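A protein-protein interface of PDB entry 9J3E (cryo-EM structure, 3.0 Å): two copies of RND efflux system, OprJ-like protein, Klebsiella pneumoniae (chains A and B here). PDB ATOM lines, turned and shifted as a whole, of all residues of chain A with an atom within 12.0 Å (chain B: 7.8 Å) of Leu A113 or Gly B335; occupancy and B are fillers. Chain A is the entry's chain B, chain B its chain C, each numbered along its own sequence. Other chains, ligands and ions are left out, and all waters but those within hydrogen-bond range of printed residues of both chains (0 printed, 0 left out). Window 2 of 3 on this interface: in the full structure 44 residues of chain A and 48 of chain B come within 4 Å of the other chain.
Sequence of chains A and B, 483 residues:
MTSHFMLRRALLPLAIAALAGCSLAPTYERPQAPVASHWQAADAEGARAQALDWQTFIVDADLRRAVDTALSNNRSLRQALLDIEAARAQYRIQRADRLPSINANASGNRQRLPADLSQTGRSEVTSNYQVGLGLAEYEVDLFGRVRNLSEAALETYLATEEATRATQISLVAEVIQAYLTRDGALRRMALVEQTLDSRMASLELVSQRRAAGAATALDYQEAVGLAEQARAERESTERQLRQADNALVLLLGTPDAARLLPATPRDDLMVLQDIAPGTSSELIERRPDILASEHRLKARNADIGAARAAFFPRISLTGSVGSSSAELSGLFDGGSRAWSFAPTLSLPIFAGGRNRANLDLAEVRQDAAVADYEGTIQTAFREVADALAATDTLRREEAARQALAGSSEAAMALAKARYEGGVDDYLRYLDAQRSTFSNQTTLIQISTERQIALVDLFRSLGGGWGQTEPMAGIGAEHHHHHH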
ATOM      1  N   ASN A 109       3.504   4.966 -33.161  1.00  0.00           N
ATOM      2  CA  ASN A 109       4.205   4.298 -32.072  1.00  0.00           C
ATOM      3  C   ASN A 109       5.098   3.208 -32.645  1.00  0.00           C
ATOM      4  O   ASN A 109       4.630   2.354 -33.407  1.00  0.00           O
ATOM      5  CB  ASN A 109       3.216   3.709 -31.067  1.00  0.00           C
ATOM      6  CG  ASN A 109       3.904   2.981 -29.932  1.00  0.00           C
ATOM      7  OD1 ASN A 109       5.009   3.340 -29.528  1.00  0.00           O
ATOM      8  ND2 ASN A 109       3.249   1.953 -29.405  1.00  0.00           N
ATOM      9  N   ARG A 110       6.375   3.236 -32.276  1.00  0.00           N
ATOM     10  CA  ARG A 110       7.349   2.245 -32.713  1.00  0.00           C
ATOM     11  C   ARG A 110       8.018   1.648 -31.483  1.00  0.00           C
ATOM     12  O   ARG A 110       8.598   2.378 -30.674  1.00  0.00           O
ATOM     13  CB  ARG A 110       8.387   2.869 -33.644  1.00  0.00           C
ATOM     14  CG  ARG A 110       9.239   1.853 -34.367  1.00  0.00           C
ATOM     15  CD  ARG A 110       9.925   2.463 -35.570  1.00  0.00           C
ATOM     16  NE  ARG A 110      10.314   1.437 -36.529  1.00  0.00           N
ATOM     17  CZ  ARG A 110      10.676   1.679 -37.779  1.00  0.00           C
ATOM     18  NH1 ARG A 110      10.731   2.912 -38.258  1.00  0.00           N
ATOM     19  NH2 ARG A 110      10.985   0.658 -38.572  1.00  0.00           N
ATOM     20  N   GLN A 111       7.941   0.327 -31.348  1.00  0.00           N
ATOM     21  CA  GLN A 111       8.426  -0.344 -30.153  1.00  0.00           C
ATOM     22  C   GLN A 111       9.009  -1.696 -30.535  1.00  0.00           C
ATOM     23  O   GLN A 111       8.497  -2.376 -31.428  1.00  0.00           O
ATOM     24  CB  GLN A 111       7.300  -0.526 -29.127  1.00  0.00           C
ATOM     25  CG  GLN A 111       7.765  -0.537 -27.686  1.00  0.00           C
ATOM     26  CD  GLN A 111       8.412  -1.844 -27.289  1.00  0.00           C
ATOM     27  OE1 GLN A 111       9.632  -1.929 -27.151  1.00  0.00           O
ATOM     28  NE2 GLN A 111       7.596  -2.875 -27.101  1.00  0.00           N
ATOM     29  N   ARG A 112      10.082  -2.082 -29.847  1.00  0.00           N
ATOM     30  CA  ARG A 112      10.653  -3.406 -30.048  1.00  0.00           C
ATOM     31  C   ARG A 112      11.579  -3.729 -28.883  1.00  0.00           C
ATOM     32  O   ARG A 112      12.203  -2.835 -28.305  1.00  0.00           O
ATOM     33  CB  ARG A 112      11.400  -3.493 -31.384  1.00  0.00           C
ATOM     34  CG  ARG A 112      12.098  -4.807 -31.610  1.00  0.00           C
ATOM     35  CD  ARG A 112      11.087  -5.932 -31.708  1.00  0.00           C
ATOM     36  NE  ARG A 112      11.711  -7.248 -31.787  1.00  0.00           N
ATOM     37  CZ  ARG A 112      11.466  -8.246 -30.948  1.00  0.00           C
ATOM     38  NH1 ARG A 112      10.607  -8.115 -29.951  1.00  0.00           N
ATOM     39  NH2 ARG A 112      12.093  -9.406 -31.121  1.00  0.00           N
ATOM     40  N   LEU A 113      11.669  -5.025 -28.557  1.00  0.00           N
ATOM     41  CA  LEU A 113      12.310  -5.528 -27.346  1.00  0.00           C
ATOM     42  C   LEU A 113      13.840  -5.459 -27.365  1.00  0.00           C
ATOM     43  O   LEU A 113      14.433  -5.139 -26.327  1.00  0.00           O
ATOM     44  CB  LEU A 113      11.848  -6.965 -27.079  1.00  0.00           C
ATOM     45  CG  LEU A 113      12.209  -7.589 -25.730  1.00  0.00           C
ATOM     46  CD1 LEU A 113      11.042  -7.478 -24.763  1.00  0.00           C
ATOM     47  CD2 LEU A 113      12.629  -9.039 -25.904  1.00  0.00           C
ATOM     48  N   PRO A 114      14.529  -5.778 -28.461  1.00  0.00           N
ATOM     49  CA  PRO A 114      15.980  -5.565 -28.508  1.00  0.00           C
ATOM     50  C   PRO A 114      16.324  -4.160 -28.995  1.00  0.00           C
ATOM     51  O   PRO A 114      15.457  -3.354 -29.325  1.00  0.00           O
ATOM     52  CB  PRO A 114      16.474  -6.640 -29.488  1.00  0.00           C
ATOM     53  CG  PRO A 114      15.278  -7.480 -29.819  1.00  0.00           C
ATOM     54  CD  PRO A 114      14.100  -6.610 -29.594  1.00  0.00           C
ATOM     55  N   ALA A 115      17.624  -3.885 -29.042  1.00  0.00           N
ATOM     56  CA  ALA A 115      18.147  -2.550 -29.295  1.00  0.00           C
ATOM     57  C   ALA A 115      18.477  -2.355 -30.770  1.00  0.00           C
ATOM     58  O   ALA A 115      18.418  -3.283 -31.580  1.00  0.00           O
ATOM     59  CB  ALA A 115      19.389  -2.293 -28.436  1.00  0.00           C
ATOM     60  N   ASP A 116      18.858  -1.118 -31.100  1.00  0.00           N
ATOM     61  CA  ASP A 116      19.110  -0.676 -32.468  1.00  0.00           C
ATOM     62  C   ASP A 116      17.850  -0.785 -33.316  1.00  0.00           C
ATOM     63  O   ASP A 116      16.788  -0.292 -32.923  1.00  0.00           O
ATOM     64  CB  ASP A 116      20.254  -1.467 -33.116  1.00  0.00           C
ATOM     65  CG  ASP A 116      21.473  -1.588 -32.218  1.00  0.00           C
ATOM     66  OD1 ASP A 116      21.389  -2.266 -31.172  1.00  0.00           O
ATOM     67  OD2 ASP A 116      22.522  -1.008 -32.566  1.00  0.00           O
ATOM     68  N   LEU A 117      17.972  -1.425 -34.476  1.00  0.00           N
ATOM     69  CA  LEU A 117      16.889  -1.601 -35.446  1.00  0.00           C
ATOM     70  C   LEU A 117      16.120  -0.298 -35.683  1.00  0.00           C
ATOM     71  O   LEU A 117      14.910  -0.195 -35.473  1.00  0.00           O
ATOM     72  CB  LEU A 117      15.951  -2.742 -35.031  1.00  0.00           C
ATOM     73  CG  LEU A 117      15.004  -2.670 -33.833  1.00  0.00           C
ATOM     74  CD1 LEU A 117      13.706  -3.284 -34.255  1.00  0.00           C
ATOM     75  CD2 LEU A 117      15.555  -3.402 -32.631  1.00  0.00           C
ATOM     76  N   SER A 118      16.848   0.705 -36.155  1.00  0.00           N
ATOM     77  CA  SER A 118      16.262   1.980 -36.536  1.00  0.00           C
ATOM     78  C   SER A 118      16.056   2.005 -38.044  1.00  0.00           C
ATOM     79  O   SER A 118      16.877   1.473 -38.799  1.00  0.00           O
ATOM     80  CB  SER A 118      17.152   3.146 -36.100  1.00  0.00           C
ATOM     81  OG  SER A 118      18.522   2.791 -36.169  1.00  0.00           O
ATOM     82  N   GLY A 121      14.833  -1.899 -39.058  1.00  0.00           N
ATOM     83  CA  GLY A 121      15.902  -2.819 -38.732  1.00  0.00           C
ATOM     84  C   GLY A 121      15.448  -4.266 -38.780  1.00  0.00           C
ATOM     85  O   GLY A 121      14.272  -4.583 -38.965  1.00  0.00           O
ATOM     86  N   ARG A 122      16.413  -5.168 -38.604  1.00  0.00           N
ATOM     87  CA  ARG A 122      16.165  -6.605 -38.727  1.00  0.00           C
ATOM     88  C   ARG A 122      15.799  -7.159 -37.356  1.00  0.00           C
ATOM     89  O   ARG A 122      16.658  -7.593 -36.587  1.00  0.00           O
ATOM     90  CB  ARG A 122      17.379  -7.321 -39.307  1.00  0.00           C
ATOM     91  CG  ARG A 122      17.776  -6.881 -40.712  1.00  0.00           C
ATOM     92  CD  ARG A 122      18.790  -5.746 -40.673  1.00  0.00           C
ATOM     93  NE  ARG A 122      19.091  -5.231 -42.003  1.00  0.00           N
ATOM     94  CZ  ARG A 122      18.352  -4.335 -42.641  1.00  0.00           C
ATOM     95  NH1 ARG A 122      17.264  -3.821 -42.093  1.00  0.00           N
ATOM     96  NH2 ARG A 122      18.715  -3.942 -43.858  1.00  0.00           N
ATOM     97  N   SER A 123      14.508  -7.150 -37.048  1.00  0.00           N
ATOM     98  CA  SER A 123      13.991  -7.682 -35.788  1.00  0.00           C
ATOM     99  C   SER A 123      12.477  -7.827 -35.924  1.00  0.00           C
ATOM    100  O   SER A 123      11.922  -7.711 -37.024  1.00  0.00           O
ATOM    101  CB  SER A 123      14.382  -6.796 -34.604  1.00  0.00           C
ATOM    102  OG  SER A 123      13.472  -6.951 -33.531  1.00  0.00           O
ATOM    103  N   GLU A 124      11.809  -8.085 -34.800  1.00  0.00           N
ATOM    104  CA  GLU A 124      10.364  -8.280 -34.763  1.00  0.00           C
ATOM    105  C   GLU A 124       9.660  -6.968 -34.436  1.00  0.00           C
ATOM    106  O   GLU A 124       8.657  -6.958 -33.714  1.00  0.00           O
ATOM    107  CB  GLU A 124      10.004  -9.360 -33.736  1.00  0.00           C
ATOM    108  CG  GLU A 124       8.658 -10.046 -33.951  1.00  0.00           C
ATOM    109  CD  GLU A 124       8.455 -11.233 -33.024  1.00  0.00           C
ATOM    110  OE1 GLU A 124       8.847 -11.141 -31.842  1.00  0.00           O
ATOM    111  OE2 GLU A 124       7.903 -12.258 -33.476  1.00  0.00           O
ATOM    112  N   VAL A 125      10.207  -5.854 -34.934  1.00  0.00           N
ATOM    113  CA  VAL A 125       9.724  -4.505 -34.642  1.00  0.00           C
ATOM    114  C   VAL A 125       8.211  -4.403 -34.781  1.00  0.00           C
ATOM    115  O   VAL A 125       7.604  -5.033 -35.656  1.00  0.00           O
ATOM    116  CB  VAL A 125      10.426  -3.457 -35.529  1.00  0.00           C
ATOM    117  CG1 VAL A 125       9.772  -3.362 -36.899  1.00  0.00           C
ATOM    118  CG2 VAL A 125      10.406  -2.100 -34.846  1.00  0.00           C
ATOM    119  N   THR A 126       7.592  -3.652 -33.880  1.00  0.00           N
ATOM    120  CA  THR A 126       6.158  -3.408 -33.911  1.00  0.00           C
ATOM    121  C   THR A 126       5.923  -1.913 -34.065  1.00  0.00           C
ATOM    122  O   THR A 126       6.083  -1.153 -33.106  1.00  0.00           O
ATOM    123  CB  THR A 126       5.490  -3.929 -32.640  1.00  0.00           C
ATOM    124  OG1 THR A 126       6.177  -5.101 -32.185  1.00  0.00           O
ATOM    125  CG2 THR A 126       4.037  -4.273 -32.913  1.00  0.00           C
ATOM    126  N   SER A 127       5.542  -1.495 -35.268  1.00  0.00           N
ATOM    127  CA  SER A 127       5.280  -0.095 -35.557  1.00  0.00           C
ATOM    128  C   SER A 127       3.793   0.082 -35.809  1.00  0.00           C
ATOM    129  O   SER A 127       3.216  -0.612 -36.650  1.00  0.00           O
ATOM    130  CB  SER A 127       6.087   0.385 -36.766  1.00  0.00           C
ATOM    131  OG  SER A 127       7.475   0.225 -36.544  1.00  0.00           O
ATOM    132  N   GLY B 322      14.869   0.856 -21.985  1.00  0.00           N
ATOM    133  CA  GLY B 322      15.197   0.057 -20.823  1.00  0.00           C
ATOM    134  C   GLY B 322      15.056  -1.425 -21.083  1.00  0.00           C
ATOM    135  O   GLY B 322      15.252  -1.882 -22.212  1.00  0.00           O
ATOM    136  N   SER B 323      14.696  -2.187 -20.055  1.00  0.00           N
ATOM    137  CA  SER B 323      14.561  -3.630 -20.165  1.00  0.00           C
ATOM    138  C   SER B 323      13.106  -4.023 -19.985  1.00  0.00           C
ATOM    139  O   SER B 323      12.312  -3.280 -19.404  1.00  0.00           O
ATOM    140  CB  SER B 323      15.423  -4.359 -19.131  1.00  0.00           C
ATOM    141  OG  SER B 323      15.289  -5.763 -19.264  1.00  0.00           O
ATOM    142  N   SER B 324      12.762  -5.200 -20.499  1.00  0.00           N
ATOM    143  CA  SER B 324      11.413  -5.726 -20.359  1.00  0.00           C
ATOM    144  C   SER B 324      11.461  -7.234 -20.543  1.00  0.00           C
ATOM    145  O   SER B 324      12.124  -7.732 -21.456  1.00  0.00           O
ATOM    146  CB  SER B 324      10.455  -5.092 -21.372  1.00  0.00           C
ATOM    147  OG  SER B 324       9.110  -5.434 -21.084  1.00  0.00           O
ATOM    148  N   SER B 325      10.760  -7.950 -19.672  1.00  0.00           N
ATOM    149  CA  SER B 325      10.738  -9.403 -19.735  1.00  0.00           C
ATOM    150  C   SER B 325       9.472  -9.897 -19.058  1.00  0.00           C
ATOM    151  O   SER B 325       8.880  -9.204 -18.227  1.00  0.00           O
ATOM    152  CB  SER B 325      11.982 -10.011 -19.078  1.00  0.00           C
ATOM    153  OG  SER B 325      11.907 -11.424 -19.054  1.00  0.00           O
ATOM    154  N   ALA B 326       9.068 -11.115 -19.418  1.00  0.00           N
ATOM    155  CA  ALA B 326       7.869 -11.708 -18.843  1.00  0.00           C
ATOM    156  C   ALA B 326       8.090 -12.222 -17.428  1.00  0.00           C
ATOM    157  O   ALA B 326       7.117 -12.558 -16.748  1.00  0.00           O
ATOM    158  CB  ALA B 326       7.364 -12.845 -19.731  1.00  0.00           C
ATOM    159  N   GLY B 330      14.706 -12.593 -15.617  1.00  0.00           N
ATOM    160  CA  GLY B 330      15.317 -12.231 -16.879  1.00  0.00           C
ATOM    161  C   GLY B 330      15.408 -10.736 -17.092  1.00  0.00           C
ATOM    162  O   GLY B 330      15.613 -10.276 -18.219  1.00  0.00           O
ATOM    163  N   LEU B 331      15.259  -9.966 -16.011  1.00  0.00           N
ATOM    164  CA  LEU B 331      15.272  -8.512 -16.133  1.00  0.00           C
ATOM    165  C   LEU B 331      16.602  -8.008 -16.676  1.00  0.00           C
ATOM    166  O   LEU B 331      16.633  -7.142 -17.558  1.00  0.00           O
ATOM    167  CB  LEU B 331      14.975  -7.869 -14.780  1.00  0.00           C
ATOM    168  CG  LEU B 331      14.825  -6.349 -14.825  1.00  0.00           C
ATOM    169  CD1 LEU B 331      13.723  -5.949 -15.796  1.00  0.00           C
ATOM    170  CD2 LEU B 331      14.564  -5.787 -13.438  1.00  0.00           C
ATOM    171  N   PHE B 332      17.713  -8.539 -16.166  1.00  0.00           N
ATOM    172  CA  PHE B 332      19.038  -8.116 -16.601  1.00  0.00           C
ATOM    173  C   PHE B 332      19.675  -9.136 -17.539  1.00  0.00           C
ATOM    174  O   PHE B 332      20.884  -9.373 -17.470  1.00  0.00           O
ATOM    175  CB  PHE B 332      19.934  -7.857 -15.388  1.00  0.00           C
ATOM    176  CG  PHE B 332      20.924  -6.738 -15.588  1.00  0.00           C
ATOM    177  CD1 PHE B 332      21.089  -5.768 -14.613  1.00  0.00           C
ATOM    178  CD2 PHE B 332      21.680  -6.648 -16.745  1.00  0.00           C
ATOM    179  CE1 PHE B 332      21.993  -4.735 -14.786  1.00  0.00           C
ATOM    180  CE2 PHE B 332      22.585  -5.622 -16.925  1.00  0.00           C
ATOM    181  CZ  PHE B 332      22.742  -4.663 -15.944  1.00  0.00           C
ATOM    182  N   ASP B 333      18.878  -9.760 -18.398  1.00  0.00           N
ATOM    183  CA  ASP B 333      19.424 -10.664 -19.393  1.00  0.00           C
ATOM    184  C   ASP B 333      19.563  -9.951 -20.734  1.00  0.00           C
ATOM    185  O   ASP B 333      18.900  -8.947 -21.007  1.00  0.00           O
ATOM    186  CB  ASP B 333      18.544 -11.905 -19.537  1.00  0.00           C
ATOM    187  CG  ASP B 333      18.675 -12.849 -18.360  1.00  0.00           C
ATOM    188  OD1 ASP B 333      19.634 -12.689 -17.576  1.00  0.00           O
ATOM    189  OD2 ASP B 333      17.825 -13.754 -18.223  1.00  0.00           O
ATOM    190  N   GLY B 334      20.447 -10.484 -21.572  1.00  0.00           N
ATOM    191  CA  GLY B 334      20.677  -9.872 -22.867  1.00  0.00           C
ATOM    192  C   GLY B 334      19.453  -9.982 -23.758  1.00  0.00           C
ATOM    193  O   GLY B 334      18.641 -10.900 -23.625  1.00  0.00           O
ATOM    194  N   GLY B 335      19.317  -9.024 -24.668  1.00  0.00           N
ATOM    195  CA  GLY B 335      18.245  -9.043 -25.637  1.00  0.00           C
ATOM    196  C   GLY B 335      16.937  -8.445 -25.177  1.00  0.00           C
ATOM    197  O   GLY B 335      15.914  -8.654 -25.840  1.00  0.00           O
ATOM    198  N   SER B 336      16.929  -7.711 -24.066  1.00  0.00           N
ATOM    199  CA  SER B 336      15.718  -7.076 -23.566  1.00  0.00           C
ATOM    200  C   SER B 336      15.788  -5.557 -23.605  1.00  0.00           C
ATOM    201  O   SER B 336      14.885  -4.898 -23.081  1.00  0.00           O
ATOM    202  CB  SER B 336      15.426  -7.542 -22.135  1.00  0.00           C
ATOM    203  OG  SER B 336      16.472  -7.173 -21.255  1.00  0.00           O
ATOM    204  N   ARG B 337      16.816  -4.986 -24.227  1.00  0.00           N
ATOM    205  CA  ARG B 337      16.989  -3.536 -24.263  1.00  0.00           C
ATOM    206  C   ARG B 337      15.958  -2.939 -25.209  1.00  0.00           C
ATOM    207  O   ARG B 337      16.234  -2.705 -26.386  1.00  0.00           O
ATOM    208  CB  ARG B 337      18.409  -3.182 -24.688  1.00  0.00           C
ATOM    209  CG  ARG B 337      19.403  -4.324 -24.537  1.00  0.00           C
ATOM    210  CD  ARG B 337      19.854  -4.455 -23.087  1.00  0.00           C
ATOM    211  NE  ARG B 337      20.689  -5.628 -22.864  1.00  0.00           N
ATOM    212  CZ  ARG B 337      21.190  -5.975 -21.685  1.00  0.00           C
ATOM    213  NH1 ARG B 337      20.956  -5.262 -20.597  1.00  0.00           N
ATOM    214  NH2 ARG B 337      21.942  -7.069 -21.597  1.00  0.00           N
ATOM    215  N   ALA B 338      14.761  -2.681 -24.689  1.00  0.00           N
ATOM    216  CA  ALA B 338      13.622  -2.235 -25.475  1.00  0.00           C
ATOM    217  C   ALA B 338      13.572  -0.716 -25.541  1.00  0.00           C
ATOM    218  O   ALA B 338      14.173  -0.014 -24.724  1.00  0.00           O
ATOM    219  CB  ALA B 338      12.313  -2.775 -24.893  1.00  0.00           C
ATOM    220  N   TRP B 339      12.846  -0.214 -26.537  1.00  0.00           N
ATOM    221  CA  TRP B 339      12.661   1.219 -26.711  1.00  0.00           C
ATOM    222  C   TRP B 339      11.294   1.483 -27.324  1.00  0.00           C
ATOM    223  O   TRP B 339      10.696   0.612 -27.959  1.00  0.00           O
ATOM    224  CB  TRP B 339      13.764   1.832 -27.580  1.00  0.00           C
ATOM    225  CG  TRP B 339      13.986   1.128 -28.880  1.00  0.00           C
ATOM    226  CD1 TRP B 339      14.965   0.221 -29.158  1.00  0.00           C
ATOM    227  CD2 TRP B 339      13.224   1.278 -30.084  1.00  0.00           C
ATOM    228  NE1 TRP B 339      14.859  -0.206 -30.458  1.00  0.00           N
ATOM    229  CE2 TRP B 339      13.797   0.428 -31.047  1.00  0.00           C
ATOM    230  CE3 TRP B 339      12.112   2.046 -30.439  1.00  0.00           C
ATOM    231  CZ2 TRP B 339      13.297   0.324 -32.342  1.00  0.00           C
ATOM    232  CZ3 TRP B 339      11.616   1.941 -31.723  1.00  0.00           C
ATOM    233  CH2 TRP B 339      12.209   1.087 -32.660  1.00  0.00           C
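The side-chain amide oxygen (OE1) of Gln A111 lies close to the backbone carbonyl oxygen (O) of Trp B339.
The backbone carbonyl oxygen of Arg A112 is in hydrogen-bond range of the backbone NH of Trp B339 (3.2 Å).
The backbone carbonyl oxygen (O) of Leu A113 sits close to the backbone NH (N) of Arg B337, 3.2 Å away.
The backbone carbonyl oxygen of Leu A113 sits at hydrogen-bond distance from the backbone NH of Ala B338, at 3.0 Å.
The indole nitrogen (NE1) of Trp B339 is in hydrogen-bond range of the backbone carbonyl oxygen (O) of Pro A114 (3.4 Å).
The backbone carbonyl oxygen of Arg B337 lies within hydrogen-bond range of the backbone NH of Ala A115.
O of Asp A116 sits at hydrogen-bond distance from NE1 of Trp B339.
The backbone carbonyl oxygen of Leu A113 sits close to the backbone carbonyl oxygen of Ser B336.
The backbone carbonyl oxygen of Pro A114 sits close to the backbone carbonyl oxygen of Arg B337.
The side-chain hydroxyl (OG) of Ser A127 is in hydrogen-bond range of the guanidinium group (NE) of Arg A110, at 3.1 Å.
N of Thr A126 sits at hydrogen-bond distance from O of Gln A111 (2.9 Å).
The guanidinium group (NH2) of Arg A112 is in salt-bridge range of the side-chain carboxylate (OE1) of Glu A124, at 3.8 Å.
The backbone NH (N) of Ala B338 is in hydrogen-bond range of the backbone carbonyl oxygen (O) of Gly B322.
The side-chain hydroxyl (OG) of Ser B323 lies within hydrogen-bond range of the side-chain hydroxyl (OG) of Ser B336, at 2.7 Å.
The backbone carbonyl oxygen of Ser B336 sits at hydrogen-bond distance from the backbone NH of Ser B324, at 3.4 Å.
Among the printed residues, pairs that only touch across the chains: Arg A110 with Trp B339 (3.2 Å), Gln A111 with Ala B338 (3.6 Å), Arg A112 with Ala B338 (3.2 Å), Leu A113 with Ser B324 (3.5 Å), Leu A113 with Gly B335 (3.3 Å) and Leu A117 with Trp B339 (3.6 Å).
Printed residues of chain B within 4 Å of Gln A111: Ala B338 (3.6 Å) and Trp B339 (2.9 Å).
Leu A113 touches just these residues of chain B: Ser B324, Gly B335, Ser B336, Arg B337 and Ala B338.
Of the printed residues of chain B, Leu A117 touches Trp B339.
No residue of chain A comes within 4 Å of Gly B322.
No residue of chain A comes within 4 Å of Ser B323.
Ser B324 touches just one residue of chain A: Leu A113.
No residue of chain A comes within 4 Å of Ser B325.
Gly B330 touches none of the printed residues of chain A.
Leu B331 touches none of the printed residues of chain A.
Gly B335 touches just one residue of chain A: Leu A113.
Ser B336 touches just one residue of chain A: Leu A113 (3.1 Å).
Arg B337 touches just these residues of chain A: Leu A113 (2.9 Å), Pro A114 (3.0 Å) and Ala A115 (3.2 Å).
Ala B338 touches just these residues of chain A: Gln A111, Arg A112 and Leu A113.
Of chain A, only Arg A110, Gln A111, Arg A112, Pro A114, Asp A116 and Leu A117 come within 4 Å of Trp B339.
The nearest residue of chain B that does not touch Leu A113 is Ser B325 (5.1 Å).
Hydrophobic or aromatic side chains of chain A within 4 Å of the printed part of chain B: Leu A113, Ala A115 and Leu A117.
Of the 15 printed residues of chain B, 6 touch a printed residue of chain A.
Along chain B the printed residues that touch a printed residue of chain A span positions 324 to 339.
Among the printed residues, 15 pairs touch across the chains.
Among the printed residues, no Asp or Glu carboxylate lies within 4 Å of a Lys or Arg side-chain nitrogen of the other chain.
No position is printed for both chains.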
